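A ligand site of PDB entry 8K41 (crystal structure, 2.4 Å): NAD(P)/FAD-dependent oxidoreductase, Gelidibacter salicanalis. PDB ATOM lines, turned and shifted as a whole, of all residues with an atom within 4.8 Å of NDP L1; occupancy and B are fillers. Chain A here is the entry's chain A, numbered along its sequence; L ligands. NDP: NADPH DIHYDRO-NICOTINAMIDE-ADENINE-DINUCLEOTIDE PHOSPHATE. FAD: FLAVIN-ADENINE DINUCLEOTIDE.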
ATOM      1  N   LYS A  57      12.376 -34.363  21.539  1.00  0.00           N
ATOM      2  CA  LYS A  57      11.018 -34.712  21.045  1.00  0.00           C
ATOM      3  C   LYS A  57      11.124 -35.608  19.790  1.00  0.00           C
ATOM      4  O   LYS A  57      10.618 -36.743  19.826  1.00  0.00           O
ATOM      5  CB  LYS A  57      10.274 -33.404  20.782  1.00  0.00           C
ATOM      6  CG  LYS A  57       8.895 -33.531  20.153  1.00  0.00           C
ATOM      7  CD  LYS A  57       8.338 -32.194  19.701  1.00  0.00           C
ATOM      8  CE  LYS A  57       8.933 -31.675  18.409  1.00  0.00           C
ATOM      9  NZ  LYS A  57       8.755 -30.211  18.295  1.00  0.00           N
ATOM     10  N   PHE A 153      -3.295 -19.566  39.029  1.00  0.00           N
ATOM     11  CA  PHE A 153      -4.453 -20.056  39.808  1.00  0.00           C
ATOM     12  C   PHE A 153      -4.033 -21.148  40.798  1.00  0.00           C
ATOM     13  O   PHE A 153      -2.840 -21.533  40.846  1.00  0.00           O
ATOM     14  CB  PHE A 153      -5.547 -20.553  38.866  1.00  0.00           C
ATOM     15  CG  PHE A 153      -5.111 -21.589  37.859  1.00  0.00           C
ATOM     16  CD1 PHE A 153      -4.966 -22.926  38.226  1.00  0.00           C
ATOM     17  CD2 PHE A 153      -4.855 -21.235  36.534  1.00  0.00           C
ATOM     18  CE1 PHE A 153      -4.558 -23.876  37.310  1.00  0.00           C
ATOM     19  CE2 PHE A 153      -4.476 -22.196  35.611  1.00  0.00           C
ATOM     20  CZ  PHE A 153      -4.318 -23.511  36.001  1.00  0.00           C
ATOM     21  N   ILE A 178      -2.922 -29.042  29.758  1.00  0.00           N
ATOM     22  CA  ILE A 178      -3.623 -27.724  29.788  1.00  0.00           C
ATOM     23  C   ILE A 178      -3.188 -26.909  28.588  1.00  0.00           C
ATOM     24  O   ILE A 178      -2.047 -26.404  28.615  1.00  0.00           O
ATOM     25  CB  ILE A 178      -3.278 -26.932  31.072  1.00  0.00           C
ATOM     26  CG1 ILE A 178      -3.779 -27.655  32.310  1.00  0.00           C
ATOM     27  CG2 ILE A 178      -3.790 -25.501  30.970  1.00  0.00           C
ATOM     28  CD1 ILE A 178      -2.885 -27.494  33.519  1.00  0.00           C
ATOM     29  N   GLY A 179      -4.103 -26.692  27.640  1.00  0.00           N
ATOM     30  CA  GLY A 179      -3.894 -25.818  26.466  1.00  0.00           C
ATOM     31  C   GLY A 179      -3.671 -26.641  25.229  1.00  0.00           C
ATOM     32  O   GLY A 179      -2.795 -27.521  25.272  1.00  0.00           O
ATOM     33  N   GLY A 180      -4.477 -26.419  24.187  1.00  0.00           N
ATOM     34  CA  GLY A 180      -4.501 -27.206  22.940  1.00  0.00           C
ATOM     35  C   GLY A 180      -3.711 -26.532  21.828  1.00  0.00           C
ATOM     36  O   GLY A 180      -4.330 -26.114  20.836  1.00  0.00           O
ATOM     37  N   GLY A 181      -2.393 -26.396  22.002  1.00  0.00           N
ATOM     38  CA  GLY A 181      -1.473 -25.958  20.931  1.00  0.00           C
ATOM     39  C   GLY A 181      -0.516 -27.051  20.480  1.00  0.00           C
ATOM     40  O   GLY A 181      -0.831 -28.285  20.659  1.00  0.00           O
ATOM     41  N   TYR A 182       0.602 -26.648  19.894  1.00  0.00           N
ATOM     42  CA  TYR A 182       1.614 -27.577  19.344  1.00  0.00           C
ATOM     43  C   TYR A 182       1.861 -28.698  20.360  1.00  0.00           C
ATOM     44  O   TYR A 182       1.720 -29.886  20.023  1.00  0.00           O
ATOM     45  CB  TYR A 182       2.964 -26.899  19.086  1.00  0.00           C
ATOM     46  CG  TYR A 182       3.024 -25.774  18.083  1.00  0.00           C
ATOM     47  CD1 TYR A 182       2.650 -24.491  18.435  1.00  0.00           C
ATOM     48  CD2 TYR A 182       3.572 -25.975  16.813  1.00  0.00           C
ATOM     49  CE1 TYR A 182       2.766 -23.438  17.536  1.00  0.00           C
ATOM     50  CE2 TYR A 182       3.719 -24.922  15.912  1.00  0.00           C
ATOM     51  CZ  TYR A 182       3.301 -23.649  16.274  1.00  0.00           C
ATOM     52  OH  TYR A 182       3.394 -22.593  15.419  1.00  0.00           O
ATOM     53  N   ILE A 183       2.250 -28.312  21.569  1.00  0.00           N
ATOM     54  CA  ILE A 183       2.926 -29.210  22.556  1.00  0.00           C
ATOM     55  C   ILE A 183       1.910 -30.263  22.994  1.00  0.00           C
ATOM     56  O   ILE A 183       2.237 -31.438  22.913  1.00  0.00           O
ATOM     57  CB  ILE A 183       3.507 -28.412  23.739  1.00  0.00           C
ATOM     58  CG1 ILE A 183       4.591 -27.452  23.253  1.00  0.00           C
ATOM     59  CG2 ILE A 183       4.015 -29.367  24.808  1.00  0.00           C
ATOM     60  CD1 ILE A 183       5.303 -26.669  24.339  1.00  0.00           C
ATOM     61  N   ALA A 184       0.728 -29.825  23.425  1.00  0.00           N
ATOM     62  CA  ALA A 184      -0.388 -30.689  23.865  1.00  0.00           C
ATOM     63  C   ALA A 184      -0.608 -31.794  22.834  1.00  0.00           C
ATOM     64  O   ALA A 184      -0.796 -32.982  23.222  1.00  0.00           O
ATOM     65  CB  ALA A 184      -1.626 -29.868  24.046  1.00  0.00           C
ATOM     66  N   GLU A 186       1.370 -32.816  20.022  1.00  0.00           N
ATOM     67  CA  GLU A 186       2.586 -33.642  19.772  1.00  0.00           C
ATOM     68  C   GLU A 186       2.830 -34.604  20.933  1.00  0.00           C
ATOM     69  O   GLU A 186       3.121 -35.800  20.686  1.00  0.00           O
ATOM     70  CB  GLU A 186       3.813 -32.749  19.600  1.00  0.00           C
ATOM     71  CG  GLU A 186       3.799 -32.018  18.269  1.00  0.00           C
ATOM     72  CD  GLU A 186       4.882 -30.982  18.152  1.00  0.00           C
ATOM     73  OE1 GLU A 186       5.534 -30.696  19.170  1.00  0.00           O
ATOM     74  OE2 GLU A 186       5.083 -30.474  17.041  1.00  0.00           O
ATOM     75  N   VAL A 201      -7.199 -30.275  27.460  1.00  0.00           N
ATOM     76  CA  VAL A 201      -8.251 -29.324  27.894  1.00  0.00           C
ATOM     77  C   VAL A 201      -7.875 -27.943  27.369  1.00  0.00           C
ATOM     78  O   VAL A 201      -6.822 -27.425  27.746  1.00  0.00           O
ATOM     79  CB  VAL A 201      -8.408 -29.332  29.422  1.00  0.00           C
ATOM     80  CG1 VAL A 201      -9.492 -28.352  29.855  1.00  0.00           C
ATOM     81  CG2 VAL A 201      -8.715 -30.745  29.927  1.00  0.00           C
ATOM     82  N   HIS A 202      -8.725 -27.368  26.520  1.00  0.00           N
ATOM     83  CA  HIS A 202      -8.420 -26.144  25.746  1.00  0.00           C
ATOM     84  C   HIS A 202      -9.575 -25.172  25.910  1.00  0.00           C
ATOM     85  O   HIS A 202     -10.699 -25.649  25.708  1.00  0.00           O
ATOM     86  CB  HIS A 202      -8.193 -26.473  24.259  1.00  0.00           C
ATOM     87  CG  HIS A 202      -8.052 -25.244  23.439  1.00  0.00           C
ATOM     88  ND1 HIS A 202      -6.999 -24.391  23.596  1.00  0.00           N
ATOM     89  CD2 HIS A 202      -8.840 -24.696  22.484  1.00  0.00           C
ATOM     90  CE1 HIS A 202      -7.117 -23.386  22.759  1.00  0.00           C
ATOM     91  NE2 HIS A 202      -8.236 -23.556  22.060  1.00  0.00           N
ATOM     92  N   ARG A 203      -9.311 -23.914  26.246  1.00  0.00           N
ATOM     93  CA  ARG A 203     -10.367 -22.918  26.613  1.00  0.00           C
ATOM     94  C   ARG A 203     -11.069 -22.379  25.350  1.00  0.00           C
ATOM     95  O   ARG A 203     -12.210 -21.893  25.445  1.00  0.00           O
ATOM     96  CB  ARG A 203      -9.738 -21.765  27.402  1.00  0.00           C
ATOM     97  CG  ARG A 203      -8.764 -20.919  26.579  1.00  0.00           C
ATOM     98  CD  ARG A 203      -8.401 -19.544  27.144  1.00  0.00           C
ATOM     99  NE  ARG A 203      -7.956 -19.605  28.532  1.00  0.00           N
ATOM    100  CZ  ARG A 203      -6.800 -19.131  28.993  1.00  0.00           C
ATOM    101  NH1 ARG A 203      -5.938 -18.545  28.187  1.00  0.00           N
ATOM    102  NH2 ARG A 203      -6.524 -19.251  30.285  1.00  0.00           N
ATOM    103  N   GLU A 209      -5.210 -22.906  17.143  1.00  0.00           N
ATOM    104  CA  GLU A 209      -6.099 -21.814  16.677  1.00  0.00           C
ATOM    105  C   GLU A 209      -5.514 -21.068  15.471  1.00  0.00           C
ATOM    106  O   GLU A 209      -6.307 -20.548  14.684  1.00  0.00           O
ATOM    107  CB  GLU A 209      -6.378 -20.846  17.837  1.00  0.00           C
ATOM    108  CG  GLU A 209      -7.252 -21.464  18.911  1.00  0.00           C
ATOM    109  CD  GLU A 209      -7.582 -20.536  20.070  1.00  0.00           C
ATOM    110  OE1 GLU A 209      -8.474 -20.891  20.883  1.00  0.00           O
ATOM    111  OE2 GLU A 209      -6.952 -19.442  20.155  1.00  0.00           O
ATOM    112  N   THR A 234     -13.436 -24.995  27.634  1.00  0.00           N
ATOM    113  CA  THR A 234     -13.218 -25.316  29.079  1.00  0.00           C
ATOM    114  C   THR A 234     -11.893 -24.701  29.516  1.00  0.00           C
ATOM    115  O   THR A 234     -10.842 -25.069  28.950  1.00  0.00           O
ATOM    116  CB  THR A 234     -13.208 -26.833  29.316  1.00  0.00           C
ATOM    117  OG1 THR A 234     -14.272 -27.436  28.577  1.00  0.00           O
ATOM    118  CG2 THR A 234     -13.324 -27.206  30.775  1.00  0.00           C
ATOM    119  N   ASP A 235     -11.945 -23.756  30.459  1.00  0.00           N
ATOM    120  CA  ASP A 235     -10.762 -23.091  31.061  1.00  0.00           C
ATOM    121  C   ASP A 235     -10.351 -23.926  32.282  1.00  0.00           C
ATOM    122  O   ASP A 235     -11.234 -24.323  33.069  1.00  0.00           O
ATOM    123  CB  ASP A 235     -11.090 -21.627  31.415  1.00  0.00           C
ATOM    124  CG  ASP A 235      -9.925 -20.799  31.917  1.00  0.00           C
ATOM    125  OD1 ASP A 235      -8.776 -21.195  31.673  1.00  0.00           O
ATOM    126  OD2 ASP A 235     -10.174 -19.736  32.549  1.00  0.00           O
ATOM    127  N   VAL A 236      -9.059 -24.202  32.444  1.00  0.00           N
ATOM    128  CA  VAL A 236      -8.557 -24.886  33.660  1.00  0.00           C
ATOM    129  C   VAL A 236      -8.265 -23.828  34.735  1.00  0.00           C
ATOM    130  O   VAL A 236      -7.543 -22.849  34.427  1.00  0.00           O
ATOM    131  CB  VAL A 236      -7.363 -25.797  33.347  1.00  0.00           C
ATOM    132  CG1 VAL A 236      -6.813 -26.428  34.604  1.00  0.00           C
ATOM    133  CG2 VAL A 236      -7.751 -26.854  32.318  1.00  0.00           C
ATOM    134  N   SER A 267       0.730 -26.981  28.996  1.00  0.00           N
ATOM    135  CA  SER A 267       0.815 -26.760  27.517  1.00  0.00           C
ATOM    136  C   SER A 267       0.302 -25.379  27.127  1.00  0.00           C
ATOM    137  O   SER A 267      -0.161 -25.251  25.979  1.00  0.00           O
ATOM    138  CB  SER A 267       0.000 -27.756  26.707  1.00  0.00           C
ATOM    139  OG  SER A 267       0.055 -29.062  27.245  1.00  0.00           O
ATOM    140  N   ALA A 268       0.318 -24.414  28.047  1.00  0.00           N
ATOM    141  CA  ALA A 268      -0.540 -23.205  27.977  1.00  0.00           C
ATOM    142  C   ALA A 268       0.199 -22.028  27.328  1.00  0.00           C
ATOM    143  O   ALA A 268      -0.149 -20.868  27.634  1.00  0.00           O
ATOM    144  CB  ALA A 268      -0.968 -22.844  29.364  1.00  0.00           C
ATOM    145  N   GLY A 269       1.165 -22.297  26.462  1.00  0.00           N
ATOM    146  CA  GLY A 269       1.944 -21.220  25.830  1.00  0.00           C
ATOM    147  C   GLY A 269       3.116 -20.749  26.680  1.00  0.00           C
ATOM    148  O   GLY A 269       3.180 -21.047  27.894  1.00  0.00           O
ATOM    149  N   ARG A 270       4.022 -20.012  26.034  1.00  0.00           N
ATOM    150  CA  ARG A 270       5.428 -19.849  26.449  1.00  0.00           C
ATOM    151  C   ARG A 270       5.794 -18.377  26.363  1.00  0.00           C
ATOM    152  O   ARG A 270       6.285 -17.921  25.337  1.00  0.00           O
ATOM    153  CB  ARG A 270       6.341 -20.700  25.575  1.00  0.00           C
ATOM    154  CG  ARG A 270       5.956 -22.177  25.583  1.00  0.00           C
ATOM    155  CD  ARG A 270       7.099 -23.022  25.075  1.00  0.00           C
ATOM    156  NE  ARG A 270       7.898 -23.448  26.201  1.00  0.00           N
ATOM    157  CZ  ARG A 270       9.181 -23.192  26.379  1.00  0.00           C
ATOM    158  NH1 ARG A 270       9.873 -22.525  25.468  1.00  0.00           N
ATOM    159  NH2 ARG A 270       9.760 -23.623  27.475  1.00  0.00           N
ATOM    160  N   ASP A 310      12.856 -16.232  20.704  1.00  0.00           N
ATOM    161  CA  ASP A 310      11.613 -16.211  21.509  1.00  0.00           C
ATOM    162  C   ASP A 310      11.615 -15.021  22.494  1.00  0.00           C
ATOM    163  O   ASP A 310      10.522 -14.556  22.864  1.00  0.00           O
ATOM    164  CB  ASP A 310      11.400 -17.525  22.263  1.00  0.00           C
ATOM    165  CG  ASP A 310      11.381 -18.768  21.381  1.00  0.00           C
ATOM    166  OD1 ASP A 310      11.484 -18.600  20.139  1.00  0.00           O
ATOM    167  OD2 ASP A 310      11.258 -19.894  21.940  1.00  0.00           O
ATOM    168  N   PRO A 318       8.218 -17.993  16.892  1.00  0.00           N
ATOM    169  CA  PRO A 318       9.123 -18.526  17.910  1.00  0.00           C
ATOM    170  C   PRO A 318       9.523 -19.951  17.522  1.00  0.00           C
ATOM    171  O   PRO A 318       8.883 -20.849  17.973  1.00  0.00           O
ATOM    172  CB  PRO A 318       8.293 -18.447  19.202  1.00  0.00           C
ATOM    173  CG  PRO A 318       6.849 -18.594  18.733  1.00  0.00           C
ATOM    174  CD  PRO A 318       6.805 -17.987  17.338  1.00  0.00           C
ATOM    175  N   LEU A 319      10.569 -20.087  16.690  1.00  0.00           N
ATOM    176  CA  LEU A 319      11.058 -21.366  16.078  1.00  0.00           C
ATOM    177  C   LEU A 319      12.596 -21.366  16.000  1.00  0.00           C
ATOM    178  O   LEU A 319      13.220 -20.282  15.918  1.00  0.00           O
ATOM    179  CB  LEU A 319      10.504 -21.519  14.652  1.00  0.00           C
ATOM    180  CG  LEU A 319       8.988 -21.537  14.467  1.00  0.00           C
ATOM    181  CD1 LEU A 319       8.646 -21.238  13.019  1.00  0.00           C
ATOM    182  CD2 LEU A 319       8.375 -22.869  14.870  1.00  0.00           C
ATOM    183  N   THR A 349       6.044 -23.935   9.268  1.00  0.00           N
ATOM    184  CA  THR A 349       5.845 -24.506  10.633  1.00  0.00           C
ATOM    185  C   THR A 349       5.209 -25.881  10.565  1.00  0.00           C
ATOM    186  O   THR A 349       4.471 -26.103   9.622  1.00  0.00           O
ATOM    187  CB  THR A 349       4.823 -23.739  11.462  1.00  0.00           C
ATOM    188  OG1 THR A 349       4.873 -22.397  10.993  1.00  0.00           O
ATOM    189  CG2 THR A 349       5.087 -23.856  12.949  1.00  0.00           C
ATOM    190  N   VAL A 350       5.392 -26.691  11.595  1.00  0.00           N
ATOM    191  CA  VAL A 350       4.937 -28.107  11.622  1.00  0.00           C
ATOM    192  C   VAL A 350       4.416 -28.459  13.007  1.00  0.00           C
ATOM    193  O   VAL A 350       4.894 -27.907  13.990  1.00  0.00           O
ATOM    194  CB  VAL A 350       6.074 -29.055  11.222  1.00  0.00           C
ATOM    195  CG1 VAL A 350       5.683 -30.488  11.434  1.00  0.00           C
ATOM    196  CG2 VAL A 350       6.528 -28.796   9.792  1.00  0.00           C
ATOM    197  N   VAL A 351       3.426 -29.350  13.037  1.00  0.00           N
ATOM    198  CA  VAL A 351       2.972 -30.074  14.257  1.00  0.00           C
ATOM    199  C   VAL A 351       3.348 -31.538  14.031  1.00  0.00           C
ATOM    200  O   VAL A 351       2.776 -32.197  13.133  1.00  0.00           O
ATOM    201  CB  VAL A 351       1.476 -29.840  14.529  1.00  0.00           C
ATOM    202  CG1 VAL A 351       0.997 -30.583  15.765  1.00  0.00           C
ATOM    203  CG2 VAL A 351       1.152 -28.342  14.642  1.00  0.00           C
ATOM    204  N   PHE A 352       4.359 -31.969  14.770  1.00  0.00           N
ATOM    205  CA  PHE A 352       4.976 -33.320  14.709  1.00  0.00           C
ATOM    206  C   PHE A 352       4.055 -34.315  15.399  1.00  0.00           C
ATOM    207  O   PHE A 352       4.532 -35.180  16.162  1.00  0.00           O
ATOM    208  CB  PHE A 352       6.386 -33.245  15.308  1.00  0.00           C
ATOM    209  CG  PHE A 352       7.330 -32.536  14.382  1.00  0.00           C
ATOM    210  CD1 PHE A 352       7.863 -33.196  13.284  1.00  0.00           C
ATOM    211  CD2 PHE A 352       7.578 -31.179  14.541  1.00  0.00           C
ATOM    212  CE1 PHE A 352       8.702 -32.536  12.405  1.00  0.00           C
ATOM    213  CE2 PHE A 352       8.410 -30.520  13.649  1.00  0.00           C
ATOM    214  CZ  PHE A 352       8.974 -31.197  12.592  1.00  0.00           C
HETATM  215  PA  NDP L   1       0.132 -22.448  22.330  1.00  0.00           P
HETATM  216  O1A NDP L   1       0.315 -20.973  22.484  1.00  0.00           O
HETATM  217  O2A NDP L   1       0.484 -23.085  21.024  1.00  0.00           O
HETATM  218  O5B NDP L   1      -1.390 -22.811  22.686  1.00  0.00           O
HETATM  219  C5B NDP L   1      -1.774 -22.991  24.078  1.00  0.00           C
HETATM  220  C4B NDP L   1      -3.256 -22.755  24.229  1.00  0.00           C
HETATM  221  O4B NDP L   1      -3.630 -23.027  25.599  1.00  0.00           O
HETATM  222  C3B NDP L   1      -3.727 -21.316  23.941  1.00  0.00           C
HETATM  223  O3B NDP L   1      -4.532 -21.264  22.764  1.00  0.00           O
HETATM  224  C2B NDP L   1      -4.488 -20.907  25.210  1.00  0.00           C
HETATM  225  O2B NDP L   1      -5.736 -20.270  24.890  1.00  0.00           O
HETATM  226  C1B NDP L   1      -4.745 -22.236  25.900  1.00  0.00           C
HETATM  227  N9A NDP L   1      -4.874 -22.129  27.356  1.00  0.00           N
HETATM  228  C8A NDP L   1      -4.216 -21.244  28.180  1.00  0.00           C
HETATM  229  N7A NDP L   1      -4.553 -21.353  29.435  1.00  0.00           N
HETATM  230  C5A NDP L   1      -5.504 -22.354  29.452  1.00  0.00           C
HETATM  231  C6A NDP L   1      -6.244 -22.943  30.489  1.00  0.00           C
HETATM  232  N6A NDP L   1      -6.163 -22.555  31.757  1.00  0.00           N
HETATM  233  N1A NDP L   1      -7.114 -23.935  30.174  1.00  0.00           N
HETATM  234  C2A NDP L   1      -7.193 -24.304  28.896  1.00  0.00           C
HETATM  235  N3A NDP L   1      -6.546 -23.828  27.829  1.00  0.00           N
HETATM  236  C4A NDP L   1      -5.706 -22.843  28.178  1.00  0.00           C
HETATM  237  O3  NDP L   1       0.925 -23.254  23.480  1.00  0.00           O
HETATM  238  PN  NDP L   1       2.055 -24.414  23.498  1.00  0.00           P
HETATM  239  O1N NDP L   1       2.200 -24.929  24.894  1.00  0.00           O
HETATM  240  O2N NDP L   1       1.752 -25.403  22.416  1.00  0.00           O
HETATM  241  O5D NDP L   1       3.367 -23.553  23.134  1.00  0.00           O
HETATM  242  C5D NDP L   1       3.885 -23.399  21.782  1.00  0.00           C
HETATM  243  C4D NDP L   1       5.289 -22.820  21.826  1.00  0.00           C
HETATM  244  O4D NDP L   1       6.262 -23.877  21.617  1.00  0.00           O
HETATM  245  C3D NDP L   1       5.644 -21.787  20.745  1.00  0.00           C
HETATM  246  O3D NDP L   1       6.771 -21.025  21.168  1.00  0.00           O
HETATM  247  C2D NDP L   1       5.986 -22.705  19.579  1.00  0.00           C
HETATM  248  O2D NDP L   1       6.781 -22.104  18.567  1.00  0.00           O
HETATM  249  C1D NDP L   1       6.737 -23.832  20.280  1.00  0.00           C
HETATM  250  N1N NDP L   1       6.492 -25.170  19.663  1.00  0.00           N
HETATM  251  C2N NDP L   1       6.767 -25.388  18.328  1.00  0.00           C
HETATM  252  C3N NDP L   1       6.621 -26.631  17.754  1.00  0.00           C
HETATM  253  C7N NDP L   1       6.877 -26.837  16.299  1.00  0.00           C
HETATM  254  O7N NDP L   1       7.263 -25.899  15.598  1.00  0.00           O
HETATM  255  N7N NDP L   1       6.672 -28.055  15.821  1.00  0.00           N
HETATM  256  C4N NDP L   1       6.193 -27.769  18.624  1.00  0.00           C
HETATM  257  C5N NDP L   1       6.038 -27.434  20.036  1.00  0.00           C
HETATM  258  C6N NDP L   1       5.966 -26.186  20.424  1.00  0.00           C
HETATM  259  P2B NDP L   1      -5.597 -18.700  24.525  1.00  0.00           P
HETATM  260  O1X NDP L   1      -4.682 -18.572  23.317  1.00  0.00           O
HETATM  261  O2X NDP L   1      -7.047 -18.447  24.185  1.00  0.00           O
HETATM  262  O3X NDP L   1      -5.106 -17.844  25.690  1.00  0.00           O
HETATM  263  PA  FAD L   2      16.547 -20.847  23.633  1.00  0.00           P
HETATM  264  O1A FAD L   2      16.993 -21.826  22.584  1.00  0.00           O
HETATM  265  O2A FAD L   2      15.608 -21.315  24.701  1.00  0.00           O
HETATM  266  O5B FAD L   2      17.835 -20.206  24.308  1.00  0.00           O
HETATM  267  C5B FAD L   2      17.638 -19.319  25.444  1.00  0.00           C
HETATM  268  C4B FAD L   2      18.526 -19.724  26.583  1.00  0.00           C
HETATM  269  O4B FAD L   2      18.410 -18.694  27.597  1.00  0.00           O
HETATM  270  C3B FAD L   2      18.197 -21.052  27.306  1.00  0.00           C
HETATM  271  O3B FAD L   2      19.308 -21.943  27.291  1.00  0.00           O
HETATM  272  C2B FAD L   2      17.798 -20.628  28.727  1.00  0.00           C
HETATM  273  O2B FAD L   2      18.159 -21.537  29.762  1.00  0.00           O
HETATM  274  C1B FAD L   2      18.543 -19.319  28.862  1.00  0.00           C
HETATM  275  N9A FAD L   2      17.993 -18.416  29.845  1.00  0.00           N
HETATM  276  C8A FAD L   2      16.673 -18.095  30.037  1.00  0.00           C
HETATM  277  N7A FAD L   2      16.495 -17.221  30.991  1.00  0.00           N
HETATM  278  C5A FAD L   2      17.770 -16.925  31.455  1.00  0.00           C
HETATM  279  C6A FAD L   2      18.241 -16.070  32.469  1.00  0.00           C
HETATM  280  N6A FAD L   2      17.468 -15.305  33.222  1.00  0.00           N
HETATM  281  N1A FAD L   2      19.589 -16.023  32.657  1.00  0.00           N
HETATM  282  C2A FAD L   2      20.370 -16.780  31.875  1.00  0.00           C
HETATM  283  N3A FAD L   2      20.028 -17.640  30.919  1.00  0.00           N
HETATM  284  C4A FAD L   2      18.696 -17.656  30.743  1.00  0.00           C
HETATM  285  N1  FAD L   2      10.968 -24.851  17.174  1.00  0.00           N
HETATM  286  C2  FAD L   2      11.092 -25.455  15.937  1.00  0.00           C
HETATM  287  O2  FAD L   2      11.486 -24.847  14.946  1.00  0.00           O
HETATM  288  N3  FAD L   2      10.771 -26.745  15.733  1.00  0.00           N
HETATM  289  C4  FAD L   2      10.316 -27.534  16.739  1.00  0.00           C
HETATM  290  O4  FAD L   2      10.031 -28.685  16.504  1.00  0.00           O
HETATM  291  C4X FAD L   2      10.203 -26.974  18.055  1.00  0.00           C
HETATM  292  N5  FAD L   2       9.790 -27.755  19.020  1.00  0.00           N
HETATM  293  C5X FAD L   2       9.734 -27.219  20.280  1.00  0.00           C
HETATM  294  C6  FAD L   2       9.323 -28.075  21.324  1.00  0.00           C
HETATM  295  C7  FAD L   2       9.247 -27.636  22.627  1.00  0.00           C
HETATM  296  C7M FAD L   2       8.814 -28.589  23.722  1.00  0.00           C
HETATM  297  C8  FAD L   2       9.533 -26.281  22.911  1.00  0.00           C
HETATM  298  C8M FAD L   2       9.425 -25.765  24.325  1.00  0.00           C
HETATM  299  C9  FAD L   2       9.917 -25.424  21.891  1.00  0.00           C
HETATM  300  C9A FAD L   2      10.033 -25.874  20.558  1.00  0.00           C
HETATM  301  N10 FAD L   2      10.431 -25.050  19.492  1.00  0.00           N
HETATM  302  C10 FAD L   2      10.548 -25.588  18.197  1.00  0.00           C
HETATM  303  C1' FAD L   2      10.780 -23.637  19.728  1.00  0.00           C
HETATM  304  C2' FAD L   2      12.289 -23.443  19.848  1.00  0.00           C
HETATM  305  O2' FAD L   2      12.822 -24.187  20.920  1.00  0.00           O
HETATM  306  C3' FAD L   2      12.695 -21.991  20.065  1.00  0.00           C
HETATM  307  O3' FAD L   2      12.085 -21.185  19.040  1.00  0.00           O
HETATM  308  C4' FAD L   2      14.217 -21.763  20.093  1.00  0.00           C
HETATM  309  O4' FAD L   2      14.818 -22.559  21.115  1.00  0.00           O
HETATM  310  C5' FAD L   2      14.544 -20.295  20.256  1.00  0.00           C
HETATM  311  O5' FAD L   2      15.958 -20.042  20.522  1.00  0.00           O
HETATM  312  P   FAD L   2      16.393 -18.884  21.558  1.00  0.00           P
HETATM  313  O1P FAD L   2      17.881 -18.914  21.479  1.00  0.00           O
HETATM  314  O2P FAD L   2      15.613 -17.621  21.392  1.00  0.00           O
HETATM  315  O3P FAD L   2      15.931 -19.546  22.949  1.00  0.00           O
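An oxygen (O4) of FAD L2 lies within hydrogen-bond range of the side-chain amino group of Lys 57 (2.7 Å).
N of Gly 269 sits at hydrogen-bond distance from O3 of NDP L1 (3.1 Å).
OD1 of Asp 235 sits at hydrogen-bond distance from N6A of NDP L1 (2.9 Å).
N1A of NDP L1 is in hydrogen-bond range of N of Val 236 (3.0 Å).
The backbone carbonyl oxygen (O) of Ser 267 sits close to an oxygen (O1N) of NDP L1 (2.6 Å).
The backbone carbonyl oxygen (O) of Pro 318 lies close to an oxygen (O3') of FAD L2, at 3.4 Å.
N7N of NDP L1 is in hydrogen-bond range of O of Val 350 (2.6 Å).
An oxygen (O2N) of NDP L1 sits at hydrogen-bond distance from the backbone NH of Ile 183 (3.1 Å).
The backbone NH (N) of Asp 310 sits at hydrogen-bond distance from an oxygen (O2P) of FAD L2.
The backbone NH (N) of Leu 319 is in hydrogen-bond range of an oxygen (O3') of FAD L2 (3.0 Å).
OE2 of Glu 186 lies within hydrogen-bond range of N7N of NDP L1 (3.1 Å).
The backbone carbonyl oxygen of Val 236 sits at hydrogen-bond distance from a nitrogen (N6A) of NDP L1, at 3.0 Å.
The backbone carbonyl oxygen of Pro 318 lies within hydrogen-bond range of an oxygen (O2D) of NDP L1, at 2.5 Å.
N3A of NDP L1 is in hydrogen-bond range of N of Arg 203 (3.2 Å).
The backbone carbonyl oxygen (O) of Leu 319 lies close to an oxygen (O3') of FAD L2 (3.4 Å).
The guanidinium group (NH1) of Arg 203 lies within salt-bridge range of an oxygen (O3X) of NDP L1.
N of Tyr 182 sits at hydrogen-bond distance from O2N of NDP L1, 3.0 Å away.
O3' of FAD L2 sits at hydrogen-bond distance from OD1 of Asp 310, at 2.9 Å.
A nitrogen (N7N) of NDP L1 sits at hydrogen-bond distance from an oxygen (O4) of FAD L2.
The backbone NH (N) of Gly 180 sits at hydrogen-bond distance from a ring nitrogen (ND1) of His 202 (3.3 Å).
OE2 of Glu 186 sits at hydrogen-bond distance from N of Phe 352.
The backbone carbonyl oxygen (O) of Ile 178 sits at hydrogen-bond distance from the backbone NH (N) of Ala 268, 3.1 Å away.
The backbone NH of Gly 179 lies within hydrogen-bond range of the backbone carbonyl oxygen of Val 201 (2.8 Å).
The side-chain carboxylate of Glu 209 sits at hydrogen-bond distance from a ring nitrogen (NE2) of His 202 (2.9 Å).
N of Arg 203 sits close to O of Thr 234, at 3.3 Å.
The guanidinium group (NH2) of Arg 203 is in salt-bridge range of the side-chain carboxylate (OD1) of Asp 235, 3.3 Å away.
O of His 202 lies within hydrogen-bond range of N of Thr 234 (3.4 Å).
NZ of Lys 57 touches C4N of NDP L1, 3.6 Å away.
Ile 178 touches NDP L1.
CA of Gly 179 touches O4B of NDP L1, 2.9 Å away.
Gly 180 touches NDP L1 (N to O4B, 3.8 Å).
Gly 181 touches NDP L1.
O of Val 201 touches C2A of NDP L1, 3.3 Å away.
His 202 touches NDP L1.
OE2 of Glu 209 touches O1X of NDP L1 (3.99 Å).
Thr 234 touches NDP L1.
Ala 268 touches NDP L1 (N to O1N, 3.7 Å).
Arg 270 touches NDP L1 (CD to O4D, 3.7 Å).
Leu 319 touches NDP L1.
Thr 349 touches NDP L1 (CG2 to O7N, 3.99 Å).
CD2 of Phe 352 touches N7N of NDP L1, at 3.5 Å.
Of the 28 residues printed, 24 come within 4 Å of NDP L1.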
